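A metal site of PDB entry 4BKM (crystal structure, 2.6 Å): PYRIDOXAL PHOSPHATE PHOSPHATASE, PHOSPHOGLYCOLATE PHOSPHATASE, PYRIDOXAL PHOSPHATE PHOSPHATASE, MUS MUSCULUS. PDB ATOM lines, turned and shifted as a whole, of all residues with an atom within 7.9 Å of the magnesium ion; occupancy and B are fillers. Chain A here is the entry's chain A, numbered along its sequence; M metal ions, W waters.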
ATOM      1  N   ASP A  29     -19.812  23.343 -21.008  1.00  0.00           N
ATOM      2  CA  ASP A  29     -20.062  24.003 -22.281  1.00  0.00           C
ATOM      3  C   ASP A  29     -21.534  23.725 -22.619  1.00  0.00           C
ATOM      4  O   ASP A  29     -22.092  22.717 -22.179  1.00  0.00           O
ATOM      5  CB  ASP A  29     -19.140  23.459 -23.374  1.00  0.00           C
ATOM      6  CG  ASP A  29     -19.525  23.957 -24.754  1.00  0.00           C
ATOM      7  OD1 ASP A  29     -19.886  25.156 -24.882  1.00  0.00           O
ATOM      8  OD2 ASP A  29     -19.468  23.153 -25.714  1.00  0.00           O
ATOM      9  N   CYS A  30     -22.175  24.613 -23.373  1.00  0.00           N
ATOM     10  CA  CYS A  30     -23.606  24.440 -23.646  1.00  0.00           C
ATOM     11  C   CYS A  30     -23.899  23.640 -24.913  1.00  0.00           C
ATOM     12  O   CYS A  30     -24.514  22.583 -24.857  1.00  0.00           O
ATOM     13  CB  CYS A  30     -24.299  25.801 -23.724  1.00  0.00           C
ATOM     14  SG  CYS A  30     -24.117  26.793 -22.240  1.00  0.00           S
ATOM     15  N   ASP A  31     -23.422  24.124 -26.056  1.00  0.00           N
ATOM     16  CA  ASP A  31     -23.750  23.498 -27.334  1.00  0.00           C
ATOM     17  C   ASP A  31     -23.024  22.170 -27.502  1.00  0.00           C
ATOM     18  O   ASP A  31     -21.808  22.095 -27.371  1.00  0.00           O
ATOM     19  CB  ASP A  31     -23.394  24.440 -28.483  1.00  0.00           C
ATOM     20  CG  ASP A  31     -24.247  25.690 -28.513  1.00  0.00           C
ATOM     21  OD1 ASP A  31     -25.433  25.609 -28.128  1.00  0.00           O
ATOM     22  OD2 ASP A  31     -23.728  26.757 -28.901  1.00  0.00           O
ATOM     23  N   GLY A  32     -23.815  21.137 -27.785  1.00  0.00           N
ATOM     24  CA  GLY A  32     -23.285  19.789 -27.966  1.00  0.00           C
ATOM     25  C   GLY A  32     -23.197  19.023 -26.661  1.00  0.00           C
ATOM     26  O   GLY A  32     -22.782  17.867 -26.650  1.00  0.00           O
ATOM     27  N   VAL A  33     -23.608  19.663 -25.566  1.00  0.00           N
ATOM     28  CA  VAL A  33     -23.499  19.069 -24.242  1.00  0.00           C
ATOM     29  C   VAL A  33     -24.861  18.993 -23.577  1.00  0.00           C
ATOM     30  O   VAL A  33     -25.312  17.919 -23.170  1.00  0.00           O
ATOM     31  CB  VAL A  33     -22.537  19.895 -23.366  1.00  0.00           C
ATOM     32  CG1 VAL A  33     -22.424  19.309 -21.973  1.00  0.00           C
ATOM     33  CG2 VAL A  33     -21.176  19.982 -24.040  1.00  0.00           C
ATOM     34  N   LEU A  34     -25.526  20.139 -23.448  1.00  0.00           N
ATOM     35  CA  LEU A  34     -26.861  20.193 -22.897  1.00  0.00           C
ATOM     36  C   LEU A  34     -27.890  20.050 -24.009  1.00  0.00           C
ATOM     37  O   LEU A  34     -29.009  19.595 -23.784  1.00  0.00           O
ATOM     38  CB  LEU A  34     -27.095  21.508 -22.163  1.00  0.00           C
ATOM     39  CG  LEU A  34     -26.186  21.793 -20.973  1.00  0.00           C
ATOM     40  CD1 LEU A  34     -26.676  23.027 -20.220  1.00  0.00           C
ATOM     41  CD2 LEU A  34     -26.110  20.596 -20.037  1.00  0.00           C
ATOM     42  N   TRP A  35     -27.505  20.447 -25.222  1.00  0.00           N
ATOM     43  CA  TRP A  35     -28.440  20.436 -26.348  1.00  0.00           C
ATOM     44  C   TRP A  35     -27.737  20.593 -27.690  1.00  0.00           C
ATOM     45  O   TRP A  35     -26.595  21.063 -27.778  1.00  0.00           O
ATOM     46  CB  TRP A  35     -29.457  21.560 -26.178  1.00  0.00           C
ATOM     47  CG  TRP A  35     -28.827  22.922 -26.049  1.00  0.00           C
ATOM     48  CD1 TRP A  35     -28.109  23.591 -27.008  1.00  0.00           C
ATOM     49  CD2 TRP A  35     -28.867  23.776 -24.903  1.00  0.00           C
ATOM     50  NE1 TRP A  35     -27.696  24.809 -26.518  1.00  0.00           N
ATOM     51  CE2 TRP A  35     -28.150  24.946 -25.227  1.00  0.00           C
ATOM     52  CE3 TRP A  35     -29.436  23.672 -23.625  1.00  0.00           C
ATOM     53  CZ2 TRP A  35     -27.990  25.999 -24.328  1.00  0.00           C
ATOM     54  CZ3 TRP A  35     -29.272  24.719 -22.748  1.00  0.00           C
ATOM     55  CH2 TRP A  35     -28.559  25.871 -23.095  1.00  0.00           C
ATOM     56  N   ASN A  36     -28.440  20.181 -28.746  1.00  0.00           N
ATOM     57  CA  ASN A  36     -28.026  20.464 -30.119  1.00  0.00           C
ATOM     58  C   ASN A  36     -29.162  21.206 -30.815  1.00  0.00           C
ATOM     59  O   ASN A  36     -30.156  20.606 -31.211  1.00  0.00           O
ATOM     60  CB  ASN A  36     -27.696  19.175 -30.877  1.00  0.00           C
ATOM     61  CG  ASN A  36     -26.360  18.590 -30.473  1.00  0.00           C
ATOM     62  OD1 ASN A  36     -25.303  19.118 -30.830  1.00  0.00           O
ATOM     63  ND2 ASN A  36     -26.386  17.482 -29.738  1.00  0.00           N
ATOM     64  N   VAL A  61     -20.202  27.788 -19.477  1.00  0.00           N
ATOM     65  CA  VAL A  61     -19.283  28.632 -20.236  1.00  0.00           C
ATOM     66  C   VAL A  61     -19.544  28.490 -21.738  1.00  0.00           C
ATOM     67  O   VAL A  61     -19.763  27.396 -22.241  1.00  0.00           O
ATOM     68  CB  VAL A  61     -17.819  28.274 -19.912  1.00  0.00           C
ATOM     69  CG1 VAL A  61     -17.556  26.807 -20.221  1.00  0.00           C
ATOM     70  CG2 VAL A  61     -16.872  29.181 -20.685  1.00  0.00           C
ATOM     71  N   PRO A 196     -21.317  27.396 -35.632  1.00  0.00           N
ATOM     72  CA  PRO A 196     -22.351  26.397 -35.873  1.00  0.00           C
ATOM     73  C   PRO A 196     -23.764  26.986 -35.912  1.00  0.00           C
ATOM     74  O   PRO A 196     -24.101  27.849 -35.099  1.00  0.00           O
ATOM     75  CB  PRO A 196     -22.221  25.453 -34.682  1.00  0.00           C
ATOM     76  CG  PRO A 196     -20.814  25.596 -34.244  1.00  0.00           C
ATOM     77  CD  PRO A 196     -20.477  27.047 -34.471  1.00  0.00           C
ATOM     78  N   LYS A 226     -12.899  30.072 -24.751  1.00  0.00           N
ATOM     79  CA  LYS A 226     -12.162  28.817 -24.773  1.00  0.00           C
ATOM     80  C   LYS A 226     -11.520  28.629 -26.135  1.00  0.00           C
ATOM     81  O   LYS A 226     -12.120  29.007 -27.146  1.00  0.00           O
ATOM     82  CB  LYS A 226     -13.089  27.638 -24.506  1.00  0.00           C
ATOM     83  CG  LYS A 226     -13.881  27.700 -23.212  1.00  0.00           C
ATOM     84  CD  LYS A 226     -15.091  26.778 -23.264  1.00  0.00           C
ATOM     85  CE  LYS A 226     -16.061  27.201 -24.357  1.00  0.00           C
ATOM     86  NZ  LYS A 226     -17.316  26.408 -24.347  1.00  0.00           N
ATOM     87  N   VAL A 249     -16.703  19.861 -18.579  1.00  0.00           N
ATOM     88  CA  VAL A 249     -17.465  18.986 -19.454  1.00  0.00           C
ATOM     89  C   VAL A 249     -17.775  19.710 -20.752  1.00  0.00           C
ATOM     90  O   VAL A 249     -18.397  20.778 -20.748  1.00  0.00           O
ATOM     91  CB  VAL A 249     -18.796  18.545 -18.811  1.00  0.00           C
ATOM     92  CG1 VAL A 249     -19.553  17.599 -19.735  1.00  0.00           C
ATOM     93  CG2 VAL A 249     -18.562  17.886 -17.461  1.00  0.00           C
ATOM     94  N   GLY A 250     -17.358  19.122 -21.862  1.00  0.00           N
ATOM     95  CA  GLY A 250     -17.565  19.717 -23.169  1.00  0.00           C
ATOM     96  C   GLY A 250     -17.627  18.675 -24.257  1.00  0.00           C
ATOM     97  O   GLY A 250     -17.266  17.519 -24.047  1.00  0.00           O
ATOM     98  N   ASP A 251     -18.102  19.082 -25.426  1.00  0.00           N
ATOM     99  CA  ASP A 251     -18.197  18.178 -26.562  1.00  0.00           C
ATOM    100  C   ASP A 251     -16.985  18.280 -27.497  1.00  0.00           C
ATOM    101  O   ASP A 251     -16.648  17.305 -28.164  1.00  0.00           O
ATOM    102  CB  ASP A 251     -19.473  18.435 -27.349  1.00  0.00           C
ATOM    103  CG  ASP A 251     -19.592  19.869 -27.824  1.00  0.00           C
ATOM    104  OD1 ASP A 251     -19.355  20.786 -27.013  1.00  0.00           O
ATOM    105  OD2 ASP A 251     -19.936  20.077 -29.005  1.00  0.00           O
ATOM    106  N   ARG A 252     -16.332  19.440 -27.550  1.00  0.00           N
ATOM    107  CA  ARG A 252     -15.227  19.624 -28.491  1.00  0.00           C
ATOM    108  C   ARG A 252     -13.863  19.548 -27.805  1.00  0.00           C
ATOM    109  O   ARG A 252     -13.651  20.119 -26.743  1.00  0.00           O
ATOM    110  CB  ARG A 252     -15.360  20.936 -29.263  1.00  0.00           C
ATOM    111  CG  ARG A 252     -14.336  21.041 -30.383  1.00  0.00           C
ATOM    112  CD  ARG A 252     -14.906  21.743 -31.604  1.00  0.00           C
ATOM    113  NE  ARG A 252     -14.038  21.573 -32.768  1.00  0.00           N
ATOM    114  CZ  ARG A 252     -13.013  22.357 -33.084  1.00  0.00           C
ATOM    115  NH1 ARG A 252     -12.298  22.099 -34.167  1.00  0.00           N
ATOM    116  NH2 ARG A 252     -12.702  23.398 -32.317  1.00  0.00           N
ATOM    117  N   LEU A 253     -12.929  18.841 -28.450  1.00  0.00           N
ATOM    118  CA  LEU A 253     -11.615  18.579 -27.868  1.00  0.00           C
ATOM    119  C   LEU A 253     -10.716  19.804 -27.912  1.00  0.00           C
ATOM    120  O   LEU A 253      -9.964  20.080 -26.977  1.00  0.00           O
ATOM    121  CB  LEU A 253     -10.929  17.428 -28.616  1.00  0.00           C
ATOM    122  CG  LEU A 253     -11.546  16.033 -28.482  1.00  0.00           C
ATOM    123  CD1 LEU A 253     -11.376  15.225 -29.762  1.00  0.00           C
ATOM    124  CD2 LEU A 253     -10.920  15.305 -27.314  1.00  0.00           C
ATOM    125  N   THR A 255     -11.436  22.968 -27.988  1.00  0.00           N
ATOM    126  CA  THR A 255     -11.852  24.138 -27.213  1.00  0.00           C
ATOM    127  C   THR A 255     -12.059  23.778 -25.744  1.00  0.00           C
ATOM    128  O   THR A 255     -11.376  24.325 -24.874  1.00  0.00           O
ATOM    129  CB  THR A 255     -13.159  24.759 -27.750  1.00  0.00           C
ATOM    130  OG1 THR A 255     -14.187  23.769 -27.823  1.00  0.00           O
ATOM    131  CG2 THR A 255     -12.934  25.357 -29.136  1.00  0.00           C
ATOM    132  N   ASP A 256     -12.972  22.859 -25.473  1.00  0.00           N
ATOM    133  CA  ASP A 256     -13.380  22.564 -24.105  1.00  0.00           C
ATOM    134  C   ASP A 256     -12.314  21.779 -23.351  1.00  0.00           C
ATOM    135  O   ASP A 256     -11.953  22.129 -22.226  1.00  0.00           O
ATOM    136  CB  ASP A 256     -14.684  21.760 -24.091  1.00  0.00           C
ATOM    137  CG  ASP A 256     -15.809  22.454 -24.841  1.00  0.00           C
ATOM    138  OD1 ASP A 256     -15.978  23.680 -24.671  1.00  0.00           O
ATOM    139  OD2 ASP A 256     -16.521  21.766 -25.613  1.00  0.00           O
ATOM    140  N   THR A 270     -17.992  14.616 -23.734  1.00  0.00           N
ATOM    141  CA  THR A 270     -19.280  13.996 -23.999  1.00  0.00           C
ATOM    142  C   THR A 270     -19.408  13.783 -25.509  1.00  0.00           C
ATOM    143  O   THR A 270     -19.022  14.647 -26.289  1.00  0.00           O
ATOM    144  CB  THR A 270     -20.460  14.820 -23.474  1.00  0.00           C
ATOM    145  OG1 THR A 270     -21.674  14.097 -23.662  1.00  0.00           O
ATOM    146  CG2 THR A 270     -20.541  16.162 -24.189  1.00  0.00           C
ATOM    147  N   GLY A 273     -21.703  15.597 -29.204  1.00  0.00           N
ATOM    148  CA  GLY A 273     -21.365  16.804 -29.931  1.00  0.00           C
ATOM    149  C   GLY A 273     -20.362  16.656 -31.059  1.00  0.00           C
ATOM    150  O   GLY A 273     -20.316  15.633 -31.751  1.00  0.00           O
ATOM    151  N   VAL A 274     -19.560  17.701 -31.241  1.00  0.00           N
ATOM    152  CA  VAL A 274     -18.693  17.837 -32.406  1.00  0.00           C
ATOM    153  C   VAL A 274     -17.615  16.760 -32.471  1.00  0.00           C
ATOM    154  O   VAL A 274     -17.486  16.057 -33.482  1.00  0.00           O
ATOM    155  CB  VAL A 274     -18.016  19.217 -32.426  1.00  0.00           C
ATOM    156  CG1 VAL A 274     -16.803  19.209 -33.343  1.00  0.00           C
ATOM    157  CG2 VAL A 274     -19.012  20.285 -32.875  1.00  0.00           C
ATOM    158  N   SER A 275     -16.842  16.605 -31.394  1.00  0.00           N
ATOM    159  CA  SER A 275     -15.719  15.679 -31.416  1.00  0.00           C
ATOM    160  C   SER A 275     -16.202  14.240 -31.298  1.00  0.00           C
ATOM    161  O   SER A 275     -17.280  13.971 -30.753  1.00  0.00           O
ATOM    162  CB  SER A 275     -14.746  15.974 -30.269  1.00  0.00           C
ATOM    163  OG  SER A 275     -14.060  17.193 -30.485  1.00  0.00           O
HETATM  164 MG    MG M   1     -19.449  22.509 -27.722  1.00  0.00          MG
HETATM  165  O   HOH W   1     -19.939  24.895 -28.050  1.00  0.00           O
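The side-chain amino group (NZ) of Lys 226 lies within salt-bridge range of the side-chain carboxylate (OD1) of Asp 256 (3.1 Å). The backbone NH (N) of Ser 275 sits close to the backbone carbonyl oxygen (O) of Asp 251 (3.3 Å). The backbone NH (N) of Asp 29 is in hydrogen-bond range of the backbone carbonyl oxygen (O) of Val 249 (2.9 Å). The side-chain carboxylate (OD2) of Asp 256 sits at hydrogen-bond distance from the backbone NH (N) of Asp 251, at 3.1 Å. OD1 of Asp 29 lies within salt-bridge range of NZ of Lys 226 (2.9 Å). The side-chain carboxylate of Asp 251 is in hydrogen-bond range of the backbone NH of Val 274 (3.3 Å). N of Arg 252 is in hydrogen-bond range of OD2 of Asp 256. The indole nitrogen (NE1) of Trp 35 sits at hydrogen-bond distance from the side-chain carboxylate (OD1) of Asp 31.
Residues that only touch the magnesium ion: Asp 256. Of the 22 residues printed, 4 come within 4 Å of the magnesium ion.
The magnesium ion is bound by the side-chain carboxylate (OD1) of Asp 251, the side-chain carboxylate (OD2) of Asp 29, the backbone carbonyl oxygen (O) of Asp 31 and water W1. Slightly farther from the magnesium ion lies OD2 of Asp 251 (2.8 Å).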
